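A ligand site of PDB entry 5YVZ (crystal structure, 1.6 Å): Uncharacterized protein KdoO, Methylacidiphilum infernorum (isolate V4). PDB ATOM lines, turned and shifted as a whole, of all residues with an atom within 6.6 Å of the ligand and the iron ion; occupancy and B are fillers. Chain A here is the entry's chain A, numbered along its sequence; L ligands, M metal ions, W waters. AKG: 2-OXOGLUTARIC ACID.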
ATOM      1  N   ARG A 127      20.671   8.678  -3.164  1.00  0.00           N
ATOM      2  CA  ARG A 127      20.214   8.360  -4.521  1.00  0.00           C
ATOM      3  C   ARG A 127      19.886   6.869  -4.593  1.00  0.00           C
ATOM      4  O   ARG A 127      20.781   6.038  -4.865  1.00  0.00           O
ATOM      5  CB  ARG A 127      21.269   8.753  -5.542  1.00  0.00           C
ATOM      6  CG  ARG A 127      21.797  10.161  -5.318  1.00  0.00           C
ATOM      7  CD  ARG A 127      22.646  10.639  -6.483  1.00  0.00           C
ATOM      8  NE  ARG A 127      23.195  11.962  -6.201  1.00  0.00           N
ATOM      9  CZ  ARG A 127      24.245  12.476  -6.816  1.00  0.00           C
ATOM     10  NH1 ARG A 127      24.871  11.762  -7.741  1.00  0.00           N
ATOM     11  NH2 ARG A 127      24.687  13.689  -6.513  1.00  0.00           N
ATOM     12  N   ILE A 131      20.608   3.466 -11.888  1.00  0.00           N
ATOM     13  CA  ILE A 131      21.033   4.394 -12.939  1.00  0.00           C
ATOM     14  C   ILE A 131      20.703   3.832 -14.320  1.00  0.00           C
ATOM     15  O   ILE A 131      20.256   4.569 -15.201  1.00  0.00           O
ATOM     16  CB  ILE A 131      22.544   4.695 -12.812  1.00  0.00           C
ATOM     17  CG1 ILE A 131      22.821   5.569 -11.596  1.00  0.00           C
ATOM     18  CG2 ILE A 131      23.070   5.343 -14.093  1.00  0.00           C
ATOM     19  CD1 ILE A 131      22.313   6.981 -11.739  1.00  0.00           C
ATOM     20  N   ASP A 142      23.044  12.178 -17.139  1.00  0.00           N
ATOM     21  CA  ASP A 142      24.353  12.088 -16.520  1.00  0.00           C
ATOM     22  C   ASP A 142      25.136  10.853 -16.955  1.00  0.00           C
ATOM     23  O   ASP A 142      26.218  10.605 -16.415  1.00  0.00           O
ATOM     24  CB  ASP A 142      24.222  12.151 -14.992  1.00  0.00           C
ATOM     25  CG  ASP A 142      24.173  13.588 -14.497  1.00  0.00           C
ATOM     26  OD1 ASP A 142      24.104  14.508 -15.346  1.00  0.00           O
ATOM     27  OD2 ASP A 142      24.203  13.808 -13.262  1.00  0.00           O
ATOM     28  N   HIS A 146      30.452  15.232 -18.401  1.00  0.00           N
ATOM     29  CA  HIS A 146      30.203  16.628 -18.074  1.00  0.00           C
ATOM     30  C   HIS A 146      31.034  17.019 -16.860  1.00  0.00           C
ATOM     31  O   HIS A 146      31.501  16.158 -16.108  1.00  0.00           O
ATOM     32  CB  HIS A 146      28.730  16.867 -17.762  1.00  0.00           C
ATOM     33  CG  HIS A 146      28.282  16.147 -16.528  1.00  0.00           C
ATOM     34  ND1 HIS A 146      28.041  14.785 -16.514  1.00  0.00           N
ATOM     35  CD2 HIS A 146      28.128  16.574 -15.255  1.00  0.00           C
ATOM     36  CE1 HIS A 146      27.717  14.417 -15.280  1.00  0.00           C
ATOM     37  NE2 HIS A 146      27.757  15.491 -14.500  1.00  0.00           N
ATOM     38  N   VAL A 147      31.197  18.327 -16.679  1.00  0.00           N
ATOM     39  CA  VAL A 147      31.516  18.890 -15.380  1.00  0.00           C
ATOM     40  C   VAL A 147      30.221  19.442 -14.803  1.00  0.00           C
ATOM     41  O   VAL A 147      29.270  19.748 -15.529  1.00  0.00           O
ATOM     42  CB  VAL A 147      32.616  19.974 -15.446  1.00  0.00           C
ATOM     43  CG1 VAL A 147      33.929  19.373 -15.955  1.00  0.00           C
ATOM     44  CG2 VAL A 147      32.177  21.151 -16.324  1.00  0.00           C
ATOM     45  N   ASP A 148      30.180  19.535 -13.479  1.00  0.00           N
ATOM     46  CA  ASP A 148      28.951  19.943 -12.802  1.00  0.00           C
ATOM     47  C   ASP A 148      28.725  21.437 -12.952  1.00  0.00           C
ATOM     48  O   ASP A 148      29.619  22.250 -12.687  1.00  0.00           O
ATOM     49  CB  ASP A 148      29.005  19.570 -11.326  1.00  0.00           C
ATOM     50  CG  ASP A 148      28.697  18.113 -11.082  1.00  0.00           C
ATOM     51  OD1 ASP A 148      28.390  17.383 -12.057  1.00  0.00           O
ATOM     52  OD2 ASP A 148      28.753  17.688  -9.912  1.00  0.00           O
ATOM     53  N   ALA A 149      27.516  21.774 -13.370  1.00  0.00           N
ATOM     54  CA  ALA A 149      27.059  23.150 -13.465  1.00  0.00           C
ATOM     55  C   ALA A 149      25.551  23.082 -13.401  1.00  0.00           C
ATOM     56  O   ALA A 149      24.933  22.337 -14.162  1.00  0.00           O
ATOM     57  CB  ALA A 149      27.527  23.826 -14.757  1.00  0.00           C
ATOM     58  N   PHE A 150      24.946  23.833 -12.488  1.00  0.00           N
ATOM     59  CA  PHE A 150      23.522  23.714 -12.247  1.00  0.00           C
ATOM     60  C   PHE A 150      22.833  25.021 -12.584  1.00  0.00           C
ATOM     61  O   PHE A 150      23.162  26.062 -12.002  1.00  0.00           O
ATOM     62  CB  PHE A 150      23.279  23.311 -10.794  1.00  0.00           C
ATOM     63  CG  PHE A 150      23.997  22.065 -10.410  1.00  0.00           C
ATOM     64  CD1 PHE A 150      23.575  20.831 -10.880  1.00  0.00           C
ATOM     65  CD2 PHE A 150      25.143  22.112  -9.624  1.00  0.00           C
ATOM     66  CE1 PHE A 150      24.247  19.672 -10.548  1.00  0.00           C
ATOM     67  CE2 PHE A 150      25.828  20.952  -9.295  1.00  0.00           C
ATOM     68  CZ  PHE A 150      25.373  19.733  -9.755  1.00  0.00           C
ATOM     69  N   ARG A 162      32.841  16.990  -4.167  1.00  0.00           N
ATOM     70  CA  ARG A 162      31.873  15.974  -3.748  1.00  0.00           C
ATOM     71  C   ARG A 162      32.572  14.749  -3.196  1.00  0.00           C
ATOM     72  O   ARG A 162      33.599  14.295  -3.712  1.00  0.00           O
ATOM     73  CB  ARG A 162      30.958  15.579  -4.917  1.00  0.00           C
ATOM     74  CG  ARG A 162      30.080  16.768  -5.311  1.00  0.00           C
ATOM     75  CD  ARG A 162      28.986  16.415  -6.312  1.00  0.00           C
ATOM     76  NE  ARG A 162      27.843  17.300  -6.099  1.00  0.00           N
ATOM     77  CZ  ARG A 162      26.741  17.303  -6.836  1.00  0.00           C
ATOM     78  NH1 ARG A 162      26.612  16.470  -7.856  1.00  0.00           N
ATOM     79  NH2 ARG A 162      25.753  18.138  -6.527  1.00  0.00           N
ATOM     80  N   PHE A 164      31.597  10.765  -2.402  1.00  0.00           N
ATOM     81  CA  PHE A 164      30.633   9.747  -2.813  1.00  0.00           C
ATOM     82  C   PHE A 164      30.903   8.456  -2.068  1.00  0.00           C
ATOM     83  O   PHE A 164      32.052   8.077  -1.875  1.00  0.00           O
ATOM     84  CB  PHE A 164      30.777   9.428  -4.310  1.00  0.00           C
ATOM     85  CG  PHE A 164      30.465  10.559  -5.225  1.00  0.00           C
ATOM     86  CD1 PHE A 164      29.172  10.745  -5.705  1.00  0.00           C
ATOM     87  CD2 PHE A 164      31.471  11.405  -5.667  1.00  0.00           C
ATOM     88  CE1 PHE A 164      28.887  11.789  -6.593  1.00  0.00           C
ATOM     89  CE2 PHE A 164      31.191  12.446  -6.564  1.00  0.00           C
ATOM     90  CZ  PHE A 164      29.891  12.624  -7.008  1.00  0.00           C
ATOM     91  N   ARG A 174      29.363   0.849  -8.766  1.00  0.00           N
ATOM     92  CA  ARG A 174      28.835   2.024  -9.450  1.00  0.00           C
ATOM     93  C   ARG A 174      29.782   2.336 -10.600  1.00  0.00           C
ATOM     94  O   ARG A 174      30.971   2.620 -10.379  1.00  0.00           O
ATOM     95  CB  ARG A 174      28.700   3.211  -8.514  1.00  0.00           C
ATOM     96  CG  ARG A 174      27.761   4.272  -9.078  1.00  0.00           C
ATOM     97  CD  ARG A 174      27.237   5.138  -8.003  1.00  0.00           C
ATOM     98  NE  ARG A 174      26.212   6.075  -8.475  1.00  0.00           N
ATOM     99  CZ  ARG A 174      24.900   5.877  -8.356  1.00  0.00           C
ATOM    100  NH1 ARG A 174      24.446   4.759  -7.808  1.00  0.00           N
ATOM    101  NH2 ARG A 174      24.060   6.810  -8.779  1.00  0.00           N
ATOM    102  N   SER A 175      29.250   2.298 -11.811  1.00  0.00           N
ATOM    103  CA  SER A 175      30.050   2.357 -13.039  1.00  0.00           C
ATOM    104  C   SER A 175      30.145   3.798 -13.496  1.00  0.00           C
ATOM    105  O   SER A 175      29.137   4.399 -13.892  1.00  0.00           O
ATOM    106  CB  SER A 175      29.439   1.489 -14.127  1.00  0.00           C
ATOM    107  OG  SER A 175      29.416   0.140 -13.707  1.00  0.00           O
ATOM    108  N   TRP A 176      31.347   4.358 -13.421  1.00  0.00           N
ATOM    109  CA  TRP A 176      31.631   5.703 -13.904  1.00  0.00           C
ATOM    110  C   TRP A 176      32.482   5.646 -15.155  1.00  0.00           C
ATOM    111  O   TRP A 176      33.164   4.658 -15.448  1.00  0.00           O
ATOM    112  CB  TRP A 176      32.397   6.523 -12.859  1.00  0.00           C
ATOM    113  CG  TRP A 176      31.549   7.301 -11.904  1.00  0.00           C
ATOM    114  CD1 TRP A 176      30.318   6.980 -11.433  1.00  0.00           C
ATOM    115  CD2 TRP A 176      31.900   8.555 -11.299  1.00  0.00           C
ATOM    116  NE1 TRP A 176      29.862   7.963 -10.558  1.00  0.00           N
ATOM    117  CE2 TRP A 176      30.826   8.933 -10.471  1.00  0.00           C
ATOM    118  CE3 TRP A 176      33.024   9.373 -11.388  1.00  0.00           C
ATOM    119  CZ2 TRP A 176      30.830  10.120  -9.732  1.00  0.00           C
ATOM    120  CZ3 TRP A 176      33.042  10.568 -10.655  1.00  0.00           C
ATOM    121  CH2 TRP A 176      31.947  10.910  -9.840  1.00  0.00           C
ATOM    122  N   HIS A 225      29.024  22.386 -19.958  1.00  0.00           N
ATOM    123  CA  HIS A 225      28.174  21.276 -19.563  1.00  0.00           C
ATOM    124  C   HIS A 225      27.205  20.889 -20.683  1.00  0.00           C
ATOM    125  O   HIS A 225      27.183  19.751 -21.149  1.00  0.00           O
ATOM    126  CB  HIS A 225      27.431  21.675 -18.282  1.00  0.00           C
ATOM    127  CG  HIS A 225      26.435  20.674 -17.799  1.00  0.00           C
ATOM    128  ND1 HIS A 225      25.174  20.565 -18.323  1.00  0.00           N
ATOM    129  CD2 HIS A 225      26.507  19.775 -16.781  1.00  0.00           C
ATOM    130  CE1 HIS A 225      24.508  19.613 -17.677  1.00  0.00           C
ATOM    131  NE2 HIS A 225      25.293  19.130 -16.742  1.00  0.00           N
ATOM    132  N   TRP A 251      34.760   7.825  -2.782  1.00  0.00           N
ATOM    133  CA  TRP A 251      35.688   8.585  -3.622  1.00  0.00           C
ATOM    134  C   TRP A 251      35.376  10.067  -3.521  1.00  0.00           C
ATOM    135  O   TRP A 251      34.285  10.468  -3.116  1.00  0.00           O
ATOM    136  CB  TRP A 251      35.679   8.094  -5.094  1.00  0.00           C
ATOM    137  CG  TRP A 251      34.352   8.126  -5.841  1.00  0.00           C
ATOM    138  CD1 TRP A 251      33.996   9.005  -6.829  1.00  0.00           C
ATOM    139  CD2 TRP A 251      33.270   7.192  -5.719  1.00  0.00           C
ATOM    140  NE1 TRP A 251      32.752   8.692  -7.327  1.00  0.00           N
ATOM    141  CE2 TRP A 251      32.281   7.589  -6.656  1.00  0.00           C
ATOM    142  CE3 TRP A 251      33.025   6.077  -4.906  1.00  0.00           C
ATOM    143  CZ2 TRP A 251      31.071   6.910  -6.792  1.00  0.00           C
ATOM    144  CZ3 TRP A 251      31.828   5.407  -5.049  1.00  0.00           C
ATOM    145  CH2 TRP A 251      30.851   5.829  -5.975  1.00  0.00           C
ATOM    146  N   THR A 255      33.934  17.913  -8.855  1.00  0.00           N
ATOM    147  CA  THR A 255      33.111  17.544 -10.010  1.00  0.00           C
ATOM    148  C   THR A 255      32.888  18.695 -10.985  1.00  0.00           C
ATOM    149  O   THR A 255      32.332  18.470 -12.066  1.00  0.00           O
ATOM    150  CB  THR A 255      31.762  16.992  -9.555  1.00  0.00           C
ATOM    151  OG1 THR A 255      31.140  17.920  -8.657  1.00  0.00           O
ATOM    152  CG2 THR A 255      31.953  15.655  -8.820  1.00  0.00           C
ATOM    153  N   HIS A 260      33.022  13.581 -15.932  1.00  0.00           N
ATOM    154  CA  HIS A 260      32.529  12.317 -15.405  1.00  0.00           C
ATOM    155  C   HIS A 260      31.142  12.004 -15.961  1.00  0.00           C
ATOM    156  O   HIS A 260      30.434  12.876 -16.487  1.00  0.00           O
ATOM    157  CB  HIS A 260      32.490  12.328 -13.872  1.00  0.00           C
ATOM    158  CG  HIS A 260      31.619  13.407 -13.311  1.00  0.00           C
ATOM    159  ND1 HIS A 260      31.994  14.736 -13.299  1.00  0.00           N
ATOM    160  CD2 HIS A 260      30.367  13.365 -12.808  1.00  0.00           C
ATOM    161  CE1 HIS A 260      31.013  15.458 -12.778  1.00  0.00           C
ATOM    162  NE2 HIS A 260      30.014  14.653 -12.485  1.00  0.00           N
ATOM    163  N   ALA A 261      30.777  10.732 -15.850  1.00  0.00           N
ATOM    164  CA  ALA A 261      29.469  10.225 -16.267  1.00  0.00           C
ATOM    165  C   ALA A 261      29.225   8.969 -15.463  1.00  0.00           C
ATOM    166  O   ALA A 261      30.177   8.307 -15.030  1.00  0.00           O
ATOM    167  CB  ALA A 261      29.425   9.907 -17.765  1.00  0.00           C
ATOM    168  N   VAL A 262      27.956   8.643 -15.229  1.00  0.00           N
ATOM    169  CA  VAL A 262      27.629   7.395 -14.547  1.00  0.00           C
ATOM    170  C   VAL A 262      26.778   6.545 -15.475  1.00  0.00           C
ATOM    171  O   VAL A 262      25.864   7.046 -16.136  1.00  0.00           O
ATOM    172  CB  VAL A 262      26.924   7.639 -13.193  1.00  0.00           C
ATOM    173  CG1 VAL A 262      25.639   8.431 -13.368  1.00  0.00           C
ATOM    174  CG2 VAL A 262      26.663   6.308 -12.473  1.00  0.00           C
ATOM    175  N   LYS A 264      25.800   2.927 -14.531  1.00  0.00           N
ATOM    176  CA  LYS A 264      25.088   1.840 -13.877  1.00  0.00           C
ATOM    177  C   LYS A 264      25.323   1.933 -12.380  1.00  0.00           C
ATOM    178  O   LYS A 264      26.373   2.399 -11.931  1.00  0.00           O
ATOM    179  CB  LYS A 264      25.536   0.465 -14.431  1.00  0.00           C
ATOM    180  CG  LYS A 264      25.052  -0.756 -13.675  1.00  0.00           C
ATOM    181  CD  LYS A 264      25.753  -2.016 -14.179  1.00  0.00           C
ATOM    182  CE  LYS A 264      27.205  -2.071 -13.718  1.00  0.00           C
ATOM    183  NZ  LYS A 264      27.352  -1.799 -12.260  1.00  0.00           N
ATOM    184  N   LEU A 268      23.533   5.327  -3.501  1.00  0.00           N
ATOM    185  CA  LEU A 268      24.692   6.202  -3.410  1.00  0.00           C
ATOM    186  C   LEU A 268      24.395   7.249  -2.366  1.00  0.00           C
ATOM    187  O   LEU A 268      23.287   7.799  -2.331  1.00  0.00           O
ATOM    188  CB  LEU A 268      24.959   6.869  -4.758  1.00  0.00           C
ATOM    189  CG  LEU A 268      26.094   7.887  -4.801  1.00  0.00           C
ATOM    190  CD1 LEU A 268      27.426   7.167  -4.773  1.00  0.00           C
ATOM    191  CD2 LEU A 268      25.972   8.764  -6.047  1.00  0.00           C
ATOM    192  N   GLU A 270      26.000  10.983  -1.182  1.00  0.00           N
ATOM    193  CA  GLU A 270      26.849  12.007  -1.746  1.00  0.00           C
ATOM    194  C   GLU A 270      26.772  13.228  -0.860  1.00  0.00           C
ATOM    195  O   GLU A 270      25.696  13.560  -0.355  1.00  0.00           O
ATOM    196  CB  GLU A 270      26.429  12.342  -3.187  1.00  0.00           C
ATOM    197  CG  GLU A 270      27.245  13.410  -3.891  1.00  0.00           C
ATOM    198  CD  GLU A 270      26.684  14.793  -3.629  1.00  0.00           C
ATOM    199  OE1 GLU A 270      25.455  14.940  -3.700  1.00  0.00           O
ATOM    200  OE2 GLU A 270      27.498  15.717  -3.410  1.00  0.00           O
HETATM  201  C1  AKG L   1      27.124  13.829  -9.981  1.00  0.00           C
HETATM  202  O1  AKG L   1      27.770  14.883 -10.188  1.00  0.00           O
HETATM  203  O2  AKG L   1      26.732  13.522  -8.815  1.00  0.00           O
HETATM  204  C2  AKG L   1      26.829  12.944 -11.142  1.00  0.00           C
HETATM  205  O5  AKG L   1      27.148  13.310 -12.265  1.00  0.00           O
HETATM  206  C3  AKG L   1      26.184  11.627 -10.898  1.00  0.00           C
HETATM  207  C4  AKG L   1      27.104  10.521 -10.507  1.00  0.00           C
HETATM  208  C5  AKG L   1      26.501   9.318  -9.875  1.00  0.00           C
HETATM  209  O3  AKG L   1      27.236   8.337  -9.555  1.00  0.00           O
HETATM  210  O4  AKG L   1      25.269   9.288  -9.653  1.00  0.00           O
HETATM  211 FE    FE M   1      27.921  15.370 -12.239  1.00  0.00          FE
HETATM  212  O   HOH W   1      25.856  16.159 -12.429  1.00  0.00           O
HETATM  213  O   HOH W   2      22.906  10.253 -10.085  1.00  0.00           O
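NE of Arg 174 lies within salt-bridge range of O3 of the ligand (2.7 Å).
The guanidinium group (NH1) of Arg 127 is in salt-bridge range of an oxygen (O2) of the ligand, 2.8 Å away.
The indole nitrogen of Trp 176 is in hydrogen-bond range of an oxygen (O3) of the ligand (2.8 Å).
An oxygen (O2) of the ligand is in salt-bridge range of the guanidinium group of Arg 162 (3.1 Å).
The side-chain carboxylate (OD2) of Asp 148 is in salt-bridge range of the guanidinium group (NH1) of Arg 162.
The side-chain hydroxyl (OG1) of Thr 255 is in hydrogen-bond range of the side-chain carboxylate (OD2) of Asp 148, at 2.7 Å.
The backbone NH (N) of Arg 127 lies within hydrogen-bond range of the backbone carbonyl oxygen (O) of Leu 268 (2.9 Å).
OE1 of Glu 270 lies within salt-bridge range of NH2 of Arg 127, 3.2 Å away.
OE2 of Glu 270 is in salt-bridge range of NE of Arg 162, 3.1 Å away.
O of Asp 142 is in hydrogen-bond range of N of Val 262 (2.9 Å).
N of Phe 164 lies within hydrogen-bond range of O of Trp 251 (2.8 Å).
The side-chain carboxylate (OD2) of Asp 142 lies close to an oxygen (O5) of the ligand (3.1 Å).
Residues that only touch the ligand: Phe 164 (3.5 Å), Val 262 (3.6 Å) and Leu 268 (3.7 Å).
Hydrophobic or aromatic side chains that line the ligand: His 146, Phe 164, Trp 176, His 260, Val 262 and Leu 268.
11 residues have an atom within 4 Å of the ligand: Arg 127, Asp 142, His 146, Asp 148, Arg 162, Phe 164, Arg 174, Trp 176, His 260, Val 262 and Leu 268.
Three residues have an atom within 4 Å of the iron ion: His 146, Asp 148 and His 260.
Along chain A the residues within 4 Å of the iron ion span positions 146 to 260.
The iron ion is bound by the side-chain carboxylate of Asp 148 (2.1 Å), an oxygen (O1) of the ligand (2.1 Å), an oxygen (O5) of the ligand (2.2 Å), water W1 (2.2 Å), a ring nitrogen (NE2) of His 260 (2.2 Å) and a ring nitrogen (NE2) of His 146 (2.3 Å).
The iron ion has six donor atoms within binding distance.
Water W2 bridges O4 of the ligand (2.6 Å) and NH1 of Arg 127 (3.4 Å).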
